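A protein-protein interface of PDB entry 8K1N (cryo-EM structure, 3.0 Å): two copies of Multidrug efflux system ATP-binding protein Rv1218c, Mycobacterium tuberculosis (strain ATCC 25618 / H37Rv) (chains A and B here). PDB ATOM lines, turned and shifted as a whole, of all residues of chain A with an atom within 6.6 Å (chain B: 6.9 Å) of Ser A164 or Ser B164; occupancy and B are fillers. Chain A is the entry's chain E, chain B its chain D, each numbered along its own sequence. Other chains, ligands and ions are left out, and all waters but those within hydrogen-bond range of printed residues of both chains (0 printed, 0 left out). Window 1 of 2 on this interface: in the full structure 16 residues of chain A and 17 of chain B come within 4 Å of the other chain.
The side-chain amino group (NZ) of Lys B138 sits at hydrogen-bond distance from the backbone carbonyl oxygen (O) of Gly A89, at 3.1 Å. The side-chain amino group (NZ) of Lys B138 is in salt-bridge range of the side-chain carboxylate (OE1) of Glu A161 (3.8 Å). The side-chain hydroxyl (OG) of Ser A164 is in hydrogen-bond range of the side-chain amino group (NZ) of Lys B138 (2.9 Å). NZ of Lys A138 lies within salt-bridge range of OE1 of Glu B161, at 2.9 Å. The side-chain amino group (NZ) of Lys A138 sits at hydrogen-bond distance from the side-chain hydroxyl (OG) of Ser B164. OG of Ser A164 sits at hydrogen-bond distance from OG of Ser B164, at 3.5 Å.
N of Gly A89 lies close to OD2 of Asp A160, at 3.3 Å. N of Gly B89 lies close to OD2 of Asp B160 (3.4 Å).
Among the printed residues, pairs that only touch across the chains: Ile A194 with Ile B194 (3.2 Å), Gly A165 with Glu B161 (3.4 Å), Lys A138 with Gly B89 (3.5 Å) and Glu A161 with Gly B165 (3.6 Å).
Ser A164 touches just these residues of chain B: Lys B138 and Ser B164. Ser B164 touches just these residues of chain A: Lys A138 and Ser A164. Of the printed residues of chain B, Ile A194 touches Ile B194 (3.2 Å). Of the printed residues of chain A, Gly B89 touches Lys A138 (3.5 Å). Printed residues of chain B within 4 Å of Lys A138: Gly B89 (3.5 Å), Glu B161 (2.9 Å) and Ser B164 (3.4 Å). Leu A146 touches none of the printed residues of chain B. The nearest residue of chain A that does not touch Ser B164 is Gly A165 (5.0 Å). The nearest printed residue of chain A that does not touch Glu B161 is Leu A166 (5.1 Å).
Of the 15 printed residues of chain B, 6 touch a printed residue of chain A. Hydrophobic or aromatic side chains of chain B within 4 Å of the printed part of chain A: Ile B194. Hydrophobic or aromatic side chains of chain A within 4 Å of the printed part of chain B: Ile A194. Along chain A the printed residues that touch a printed residue of chain B span positions 89 to 194. Among the printed residues, Asp or Glu carboxylates within 4 Å of a Lys or Arg side-chain nitrogen of the other chain: Lys A138 with Glu B161 (2.9 Å) and Glu A161 with Lys B138 (3.8 Å).
Gly A89 touches Lys B138, and with the chains exchanged Lys A138 touches Gly B89. Lys A138 touches Glu B161, and with the chains exchanged Glu A161 touches Lys B138. Lys A138 touches Ser B164, and with the chains exchanged Ser A164 touches Lys B138. Ser A164 touches its own counterpart, Ser B164. 14 positions are printed for both chains.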
ATOM      1  N   GLY A  89     -26.662  38.914   0.384  1.00  0.00           N
ATOM      2  CA  GLY A  89     -26.070  37.590   0.580  1.00  0.00           C
ATOM      3  C   GLY A  89     -27.053  36.553   0.170  1.00  0.00           C
ATOM      4  O   GLY A  89     -26.631  35.609  -0.480  1.00  0.00           O
ATOM      5  N   VAL A  91     -30.144  36.511  -2.108  1.00  0.00           N
ATOM      6  CA  VAL A  91     -30.986  37.194  -3.116  1.00  0.00           C
ATOM      7  C   VAL A  91     -32.388  36.597  -3.088  1.00  0.00           C
ATOM      8  O   VAL A  91     -32.524  35.436  -3.417  1.00  0.00           O
ATOM      9  CB  VAL A  91     -30.291  37.211  -4.479  1.00  0.00           C
ATOM     10  CG1 VAL A  91     -29.079  38.115  -4.501  1.00  0.00           C
ATOM     11  CG2 VAL A  91     -30.040  35.847  -5.094  1.00  0.00           C
ATOM     12  N   LYS A 138     -31.729  28.768  -8.614  1.00  0.00           N
ATOM     13  CA  LYS A 138     -30.764  29.534  -7.798  1.00  0.00           C
ATOM     14  C   LYS A 138     -29.659  29.966  -8.695  1.00  0.00           C
ATOM     15  O   LYS A 138     -29.179  31.058  -8.509  1.00  0.00           O
ATOM     16  CB  LYS A 138     -30.037  28.706  -6.757  1.00  0.00           C
ATOM     17  CG  LYS A 138     -29.253  29.500  -5.727  1.00  0.00           C
ATOM     18  CD  LYS A 138     -28.740  28.644  -4.597  1.00  0.00           C
ATOM     19  CE  LYS A 138     -28.004  27.420  -5.090  1.00  0.00           C
ATOM     20  NZ  LYS A 138     -26.593  27.426  -4.644  1.00  0.00           N
ATOM     21  N   GLY A 139     -29.274  29.269  -9.706  1.00  0.00           N
ATOM     22  CA  GLY A 139     -28.264  29.865 -10.577  1.00  0.00           C
ATOM     23  C   GLY A 139     -28.850  31.029 -11.291  1.00  0.00           C
ATOM     24  O   GLY A 139     -28.205  32.019 -11.235  1.00  0.00           O
ATOM     25  N   GLN A 142     -29.534  34.403  -8.923  1.00  0.00           N
ATOM     26  CA  GLN A 142     -28.388  35.264  -8.658  1.00  0.00           C
ATOM     27  C   GLN A 142     -28.079  36.170  -9.841  1.00  0.00           C
ATOM     28  O   GLN A 142     -27.598  37.295  -9.655  1.00  0.00           O
ATOM     29  CB  GLN A 142     -27.171  34.409  -8.311  1.00  0.00           C
ATOM     30  CG  GLN A 142     -26.028  35.170  -7.678  1.00  0.00           C
ATOM     31  CD  GLN A 142     -26.291  35.502  -6.230  1.00  0.00           C
ATOM     32  OE1 GLN A 142     -27.018  34.791  -5.542  1.00  0.00           O
ATOM     33  NE2 GLN A 142     -25.697  36.590  -5.756  1.00  0.00           N
ATOM     34  N   LEU A 146     -27.164  40.201 -10.006  1.00  0.00           N
ATOM     35  CA  LEU A 146     -25.884  40.605 -10.575  1.00  0.00           C
ATOM     36  C   LEU A 146     -26.070  41.558 -11.750  1.00  0.00           C
ATOM     37  O   LEU A 146     -25.334  42.542 -11.880  1.00  0.00           O
ATOM     38  CB  LEU A 146     -25.086  39.376 -10.995  1.00  0.00           C
ATOM     39  CG  LEU A 146     -24.365  38.646  -9.864  1.00  0.00           C
ATOM     40  CD1 LEU A 146     -23.669  37.413 -10.392  1.00  0.00           C
ATOM     41  CD2 LEU A 146     -23.375  39.570  -9.187  1.00  0.00           C
ATOM     42  N   ASP A 160     -22.032  40.809  -1.537  1.00  0.00           N
ATOM     43  CA  ASP A 160     -22.032  39.937  -0.364  1.00  0.00           C
ATOM     44  C   ASP A 160     -22.336  38.529  -0.861  1.00  0.00           C
ATOM     45  O   ASP A 160     -23.495  38.202  -1.137  1.00  0.00           O
ATOM     46  CB  ASP A 160     -23.048  40.406   0.672  1.00  0.00           C
ATOM     47  CG  ASP A 160     -23.001  39.590   1.946  1.00  0.00           C
ATOM     48  OD1 ASP A 160     -22.022  39.731   2.708  1.00  0.00           O
ATOM     49  OD2 ASP A 160     -23.948  38.821   2.199  1.00  0.00           O
ATOM     50  N   GLU A 161     -21.298  37.708  -0.972  1.00  0.00           N
ATOM     51  CA  GLU A 161     -21.370  36.415  -1.642  1.00  0.00           C
ATOM     52  C   GLU A 161     -21.941  36.583  -3.053  1.00  0.00           C
ATOM     53  O   GLU A 161     -22.996  36.031  -3.369  1.00  0.00           O
ATOM     54  CB  GLU A 161     -22.199  35.424  -0.839  1.00  0.00           C
ATOM     55  CG  GLU A 161     -21.752  35.276   0.599  1.00  0.00           C
ATOM     56  CD  GLU A 161     -22.532  34.212   1.338  1.00  0.00           C
ATOM     57  OE1 GLU A 161     -22.695  33.104   0.787  1.00  0.00           O
ATOM     58  OE2 GLU A 161     -22.983  34.483   2.470  1.00  0.00           O
ATOM     59  N   PRO A 162     -21.269  37.352  -3.912  1.00  0.00           N
ATOM     60  CA  PRO A 162     -21.871  37.693  -5.210  1.00  0.00           C
ATOM     61  C   PRO A 162     -22.121  36.500  -6.109  1.00  0.00           C
ATOM     62  O   PRO A 162     -23.101  36.507  -6.867  1.00  0.00           O
ATOM     63  CB  PRO A 162     -20.847  38.656  -5.821  1.00  0.00           C
ATOM     64  CG  PRO A 162     -19.563  38.292  -5.185  1.00  0.00           C
ATOM     65  CD  PRO A 162     -19.881  37.829  -3.801  1.00  0.00           C
ATOM     66  N   SER A 163     -21.282  35.473  -6.055  1.00  0.00           N
ATOM     67  CA  SER A 163     -21.400  34.317  -6.937  1.00  0.00           C
ATOM     68  C   SER A 163     -21.730  33.096  -6.087  1.00  0.00           C
ATOM     69  O   SER A 163     -20.850  32.341  -5.675  1.00  0.00           O
ATOM     70  CB  SER A 163     -20.131  34.119  -7.721  1.00  0.00           C
ATOM     71  OG  SER A 163     -19.135  33.514  -6.918  1.00  0.00           O
ATOM     72  N   SER A 164     -23.020  32.900  -5.838  1.00  0.00           N
ATOM     73  CA  SER A 164     -23.523  31.768  -5.069  1.00  0.00           C
ATOM     74  C   SER A 164     -24.518  31.019  -5.941  1.00  0.00           C
ATOM     75  O   SER A 164     -25.603  31.529  -6.230  1.00  0.00           O
ATOM     76  CB  SER A 164     -24.168  32.236  -3.766  1.00  0.00           C
ATOM     77  OG  SER A 164     -24.797  31.159  -3.096  1.00  0.00           O
ATOM     78  N   GLY A 165     -24.152  29.812  -6.356  1.00  0.00           N
ATOM     79  CA  GLY A 165     -24.958  29.048  -7.279  1.00  0.00           C
ATOM     80  C   GLY A 165     -24.557  29.172  -8.729  1.00  0.00           C
ATOM     81  O   GLY A 165     -25.298  28.703  -9.597  1.00  0.00           O
ATOM     82  N   LEU A 166     -23.411  29.778  -9.016  1.00  0.00           N
ATOM     83  CA  LEU A 166     -22.963  30.023 -10.378  1.00  0.00           C
ATOM     84  C   LEU A 166     -21.896  29.012 -10.770  1.00  0.00           C
ATOM     85  O   LEU A 166     -20.919  28.816 -10.041  1.00  0.00           O
ATOM     86  CB  LEU A 166     -22.402  31.440 -10.513  1.00  0.00           C
ATOM     87  CG  LEU A 166     -23.336  32.544 -11.010  1.00  0.00           C
ATOM     88  CD1 LEU A 166     -24.534  32.687 -10.106  1.00  0.00           C
ATOM     89  CD2 LEU A 166     -22.586  33.856 -11.093  1.00  0.00           C
ATOM     90  N   GLU A 171     -18.909  32.140 -13.243  1.00  0.00           N
ATOM     91  CA  GLU A 171     -17.920  32.703 -12.330  1.00  0.00           C
ATOM     92  C   GLU A 171     -16.853  33.475 -13.094  1.00  0.00           C
ATOM     93  O   GLU A 171     -16.488  34.595 -12.717  1.00  0.00           O
ATOM     94  CB  GLU A 171     -17.287  31.587 -11.502  1.00  0.00           C
ATOM     95  CG  GLU A 171     -16.095  32.026 -10.678  1.00  0.00           C
ATOM     96  CD  GLU A 171     -16.475  32.944  -9.546  1.00  0.00           C
ATOM     97  OE1 GLU A 171     -17.620  32.841  -9.062  1.00  0.00           O
ATOM     98  OE2 GLU A 171     -15.633  33.769  -9.138  1.00  0.00           O
ATOM     99  N   ILE A 194     -15.337  32.720  -0.559  1.00  0.00           N
ATOM    100  CA  ILE A 194     -14.647  31.825  -1.479  1.00  0.00           C
ATOM    101  C   ILE A 194     -13.296  32.462  -1.761  1.00  0.00           C
ATOM    102  O   ILE A 194     -13.205  33.440  -2.512  1.00  0.00           O
ATOM    103  CB  ILE A 194     -15.436  31.589  -2.769  1.00  0.00           C
ATOM    104  CG1 ILE A 194     -16.757  30.892  -2.457  1.00  0.00           C
ATOM    105  CG2 ILE A 194     -14.626  30.760  -3.740  1.00  0.00           C
ATOM    106  CD1 ILE A 194     -17.521  30.468  -3.680  1.00  0.00           C
ATOM    107  N   GLY B  89     -29.415  20.915  -4.211  1.00  0.00           N
ATOM    108  CA  GLY B  89     -28.763  22.149  -4.614  1.00  0.00           C
ATOM    109  C   GLY B  89     -29.396  23.378  -3.991  1.00  0.00           C
ATOM    110  O   GLY B  89     -28.696  24.314  -3.596  1.00  0.00           O
ATOM    111  N   LYS B 138     -28.823  31.828   5.894  1.00  0.00           N
ATOM    112  CA  LYS B 138     -28.379  31.065   4.731  1.00  0.00           C
ATOM    113  C   LYS B 138     -27.327  30.033   5.110  1.00  0.00           C
ATOM    114  O   LYS B 138     -27.363  28.896   4.628  1.00  0.00           O
ATOM    115  CB  LYS B 138     -27.841  32.012   3.662  1.00  0.00           C
ATOM    116  CG  LYS B 138     -27.417  31.330   2.378  1.00  0.00           C
ATOM    117  CD  LYS B 138     -26.944  32.348   1.360  1.00  0.00           C
ATOM    118  CE  LYS B 138     -26.494  31.671   0.081  1.00  0.00           C
ATOM    119  NZ  LYS B 138     -26.026  32.649  -0.934  1.00  0.00           N
ATOM    120  N   GLY B 139     -26.377  30.410   5.965  1.00  0.00           N
ATOM    121  CA  GLY B 139     -25.346  29.471   6.369  1.00  0.00           C
ATOM    122  C   GLY B 139     -25.877  28.343   7.232  1.00  0.00           C
ATOM    123  O   GLY B 139     -25.461  27.192   7.086  1.00  0.00           O
ATOM    124  N   ARG B 141     -28.914  27.103   7.286  1.00  0.00           N
ATOM    125  CA  ARG B 141     -29.812  26.199   6.580  1.00  0.00           C
ATOM    126  C   ARG B 141     -29.051  25.064   5.908  1.00  0.00           C
ATOM    127  O   ARG B 141     -29.556  23.940   5.834  1.00  0.00           O
ATOM    128  CB  ARG B 141     -30.625  26.970   5.546  1.00  0.00           C
ATOM    129  CG  ARG B 141     -32.015  27.345   6.001  1.00  0.00           C
ATOM    130  CD  ARG B 141     -32.806  27.959   4.865  1.00  0.00           C
ATOM    131  NE  ARG B 141     -32.549  29.389   4.735  1.00  0.00           N
ATOM    132  CZ  ARG B 141     -32.071  29.965   3.639  1.00  0.00           C
ATOM    133  NH1 ARG B 141     -31.869  31.274   3.610  1.00  0.00           N
ATOM    134  NH2 ARG B 141     -31.791  29.231   2.572  1.00  0.00           N
ATOM    135  N   GLN B 142     -27.845  25.342   5.409  1.00  0.00           N
ATOM    136  CA  GLN B 142     -27.043  24.304   4.775  1.00  0.00           C
ATOM    137  C   GLN B 142     -26.515  23.303   5.792  1.00  0.00           C
ATOM    138  O   GLN B 142     -26.345  22.120   5.469  1.00  0.00           O
ATOM    139  CB  GLN B 142     -25.889  24.942   4.007  1.00  0.00           C
ATOM    140  CG  GLN B 142     -25.201  24.020   3.027  1.00  0.00           C
ATOM    141  CD  GLN B 142     -26.008  23.809   1.770  1.00  0.00           C
ATOM    142  OE1 GLN B 142     -26.786  24.671   1.367  1.00  0.00           O
ATOM    143  NE2 GLN B 142     -25.828  22.657   1.137  1.00  0.00           N
ATOM    144  N   LEU B 146     -26.360  19.169   5.700  1.00  0.00           N
ATOM    145  CA  LEU B 146     -25.059  18.515   5.790  1.00  0.00           C
ATOM    146  C   LEU B 146     -24.996  17.557   6.975  1.00  0.00           C
ATOM    147  O   LEU B 146     -24.455  16.452   6.856  1.00  0.00           O
ATOM    148  CB  LEU B 146     -23.953  19.561   5.880  1.00  0.00           C
ATOM    149  CG  LEU B 146     -23.550  20.203   4.553  1.00  0.00           C
ATOM    150  CD1 LEU B 146     -22.498  21.264   4.779  1.00  0.00           C
ATOM    151  CD2 LEU B 146     -23.047  19.148   3.590  1.00  0.00           C
ATOM    152  N   ASP B 160     -24.709  18.055  -4.018  1.00  0.00           N
ATOM    153  CA  ASP B 160     -24.958  18.966  -5.133  1.00  0.00           C
ATOM    154  C   ASP B 160     -24.805  20.380  -4.587  1.00  0.00           C
ATOM    155  O   ASP B 160     -25.713  20.897  -3.929  1.00  0.00           O
ATOM    156  CB  ASP B 160     -26.339  18.735  -5.736  1.00  0.00           C
ATOM    157  CG  ASP B 160     -26.590  19.589  -6.963  1.00  0.00           C
ATOM    158  OD1 ASP B 160     -25.981  19.313  -8.016  1.00  0.00           O
ATOM    159  OD2 ASP B 160     -27.406  20.527  -6.882  1.00  0.00           O
ATOM    160  N   GLU B 161     -23.660  20.996  -4.865  1.00  0.00           N
ATOM    161  CA  GLU B 161     -23.254  22.248  -4.238  1.00  0.00           C
ATOM    162  C   GLU B 161     -23.318  22.117  -2.712  1.00  0.00           C
ATOM    163  O   GLU B 161     -24.075  22.835  -2.056  1.00  0.00           O
ATOM    164  CB  GLU B 161     -24.114  23.409  -4.716  1.00  0.00           C
ATOM    165  CG  GLU B 161     -24.178  23.541  -6.222  1.00  0.00           C
ATOM    166  CD  GLU B 161     -24.955  24.762  -6.660  1.00  0.00           C
ATOM    167  OE1 GLU B 161     -24.709  25.854  -6.109  1.00  0.00           O
ATOM    168  OE2 GLU B 161     -25.814  24.629  -7.556  1.00  0.00           O
ATOM    169  N   PRO B 162     -22.542  21.201  -2.130  1.00  0.00           N
ATOM    170  CA  PRO B 162     -22.705  20.911  -0.697  1.00  0.00           C
ATOM    171  C   PRO B 162     -22.403  22.087   0.211  1.00  0.00           C
ATOM    172  O   PRO B 162     -23.040  22.219   1.263  1.00  0.00           O
ATOM    173  CB  PRO B 162     -21.729  19.754  -0.466  1.00  0.00           C
ATOM    174  CG  PRO B 162     -20.705  19.911  -1.520  1.00  0.00           C
ATOM    175  CD  PRO B 162     -21.393  20.488  -2.712  1.00  0.00           C
ATOM    176  N   SER B 163     -21.461  22.947  -0.154  1.00  0.00           N
ATOM    177  CA  SER B 163     -21.049  24.063   0.691  1.00  0.00           C
ATOM    178  C   SER B 163     -21.423  25.363  -0.014  1.00  0.00           C
ATOM    179  O   SER B 163     -20.619  25.966  -0.722  1.00  0.00           O
ATOM    180  CB  SER B 163     -19.573  23.993   0.975  1.00  0.00           C
ATOM    181  OG  SER B 163     -18.825  24.447  -0.138  1.00  0.00           O
ATOM    182  N   SER B 164     -22.659  25.799   0.204  1.00  0.00           N
ATOM    183  CA  SER B 164     -23.180  27.038  -0.361  1.00  0.00           C
ATOM    184  C   SER B 164     -23.652  27.910   0.791  1.00  0.00           C
ATOM    185  O   SER B 164     -24.644  27.591   1.453  1.00  0.00           O
ATOM    186  CB  SER B 164     -24.314  26.756  -1.343  1.00  0.00           C
ATOM    187  OG  SER B 164     -24.926  27.958  -1.771  1.00  0.00           O
ATOM    188  N   GLY B 165     -22.949  29.012   1.028  1.00  0.00           N
ATOM    189  CA  GLY B 165     -23.226  29.864   2.160  1.00  0.00           C
ATOM    190  C   GLY B 165     -22.376  29.600   3.380  1.00  0.00           C
ATOM    191  O   GLY B 165     -22.666  30.154   4.444  1.00  0.00           O
ATOM    192  N   LEU B 166     -21.335  28.786   3.257  1.00  0.00           N
ATOM    193  CA  LEU B 166     -20.492  28.399   4.379  1.00  0.00           C
ATOM    194  C   LEU B 166     -19.196  29.197   4.348  1.00  0.00           C
ATOM    195  O   LEU B 166     -18.535  29.277   3.310  1.00  0.00           O
ATOM    196  CB  LEU B 166     -20.192  26.901   4.334  1.00  0.00           C
ATOM    197  CG  LEU B 166     -21.079  25.960   5.149  1.00  0.00           C
ATOM    198  CD1 LEU B 166     -22.522  26.078   4.728  1.00  0.00           C
ATOM    199  CD2 LEU B 166     -20.604  24.533   4.989  1.00  0.00           C
ATOM    200  N   GLU B 171     -16.159  25.458   5.676  1.00  0.00           N
ATOM    201  CA  GLU B 171     -15.673  24.771   4.485  1.00  0.00           C
ATOM    202  C   GLU B 171     -14.567  23.784   4.839  1.00  0.00           C
ATOM    203  O   GLU B 171     -14.570  22.637   4.380  1.00  0.00           O
ATOM    204  CB  GLU B 171     -15.174  25.792   3.466  1.00  0.00           C
ATOM    205  CG  GLU B 171     -14.446  25.187   2.283  1.00  0.00           C
ATOM    206  CD  GLU B 171     -15.361  24.407   1.375  1.00  0.00           C
ATOM    207  OE1 GLU B 171     -16.561  24.737   1.323  1.00  0.00           O
ATOM    208  OE2 GLU B 171     -14.880  23.465   0.714  1.00  0.00           O
ATOM    209  N   ILE B 194     -17.408  24.847  -7.442  1.00  0.00           N
ATOM    210  CA  ILE B 194     -16.287  25.562  -6.839  1.00  0.00           C
ATOM    211  C   ILE B 194     -15.064  24.679  -7.038  1.00  0.00           C
ATOM    212  O   ILE B 194     -14.898  23.666  -6.349  1.00  0.00           O
ATOM    213  CB  ILE B 194     -16.519  25.874  -5.359  1.00  0.00           C
ATOM    214  CG1 ILE B 194     -17.714  26.811  -5.201  1.00  0.00           C
ATOM    215  CG2 ILE B 194     -15.282  26.496  -4.750  1.00  0.00           C
ATOM    216  CD1 ILE B 194     -17.910  27.304  -3.795  1.00  0.00           C
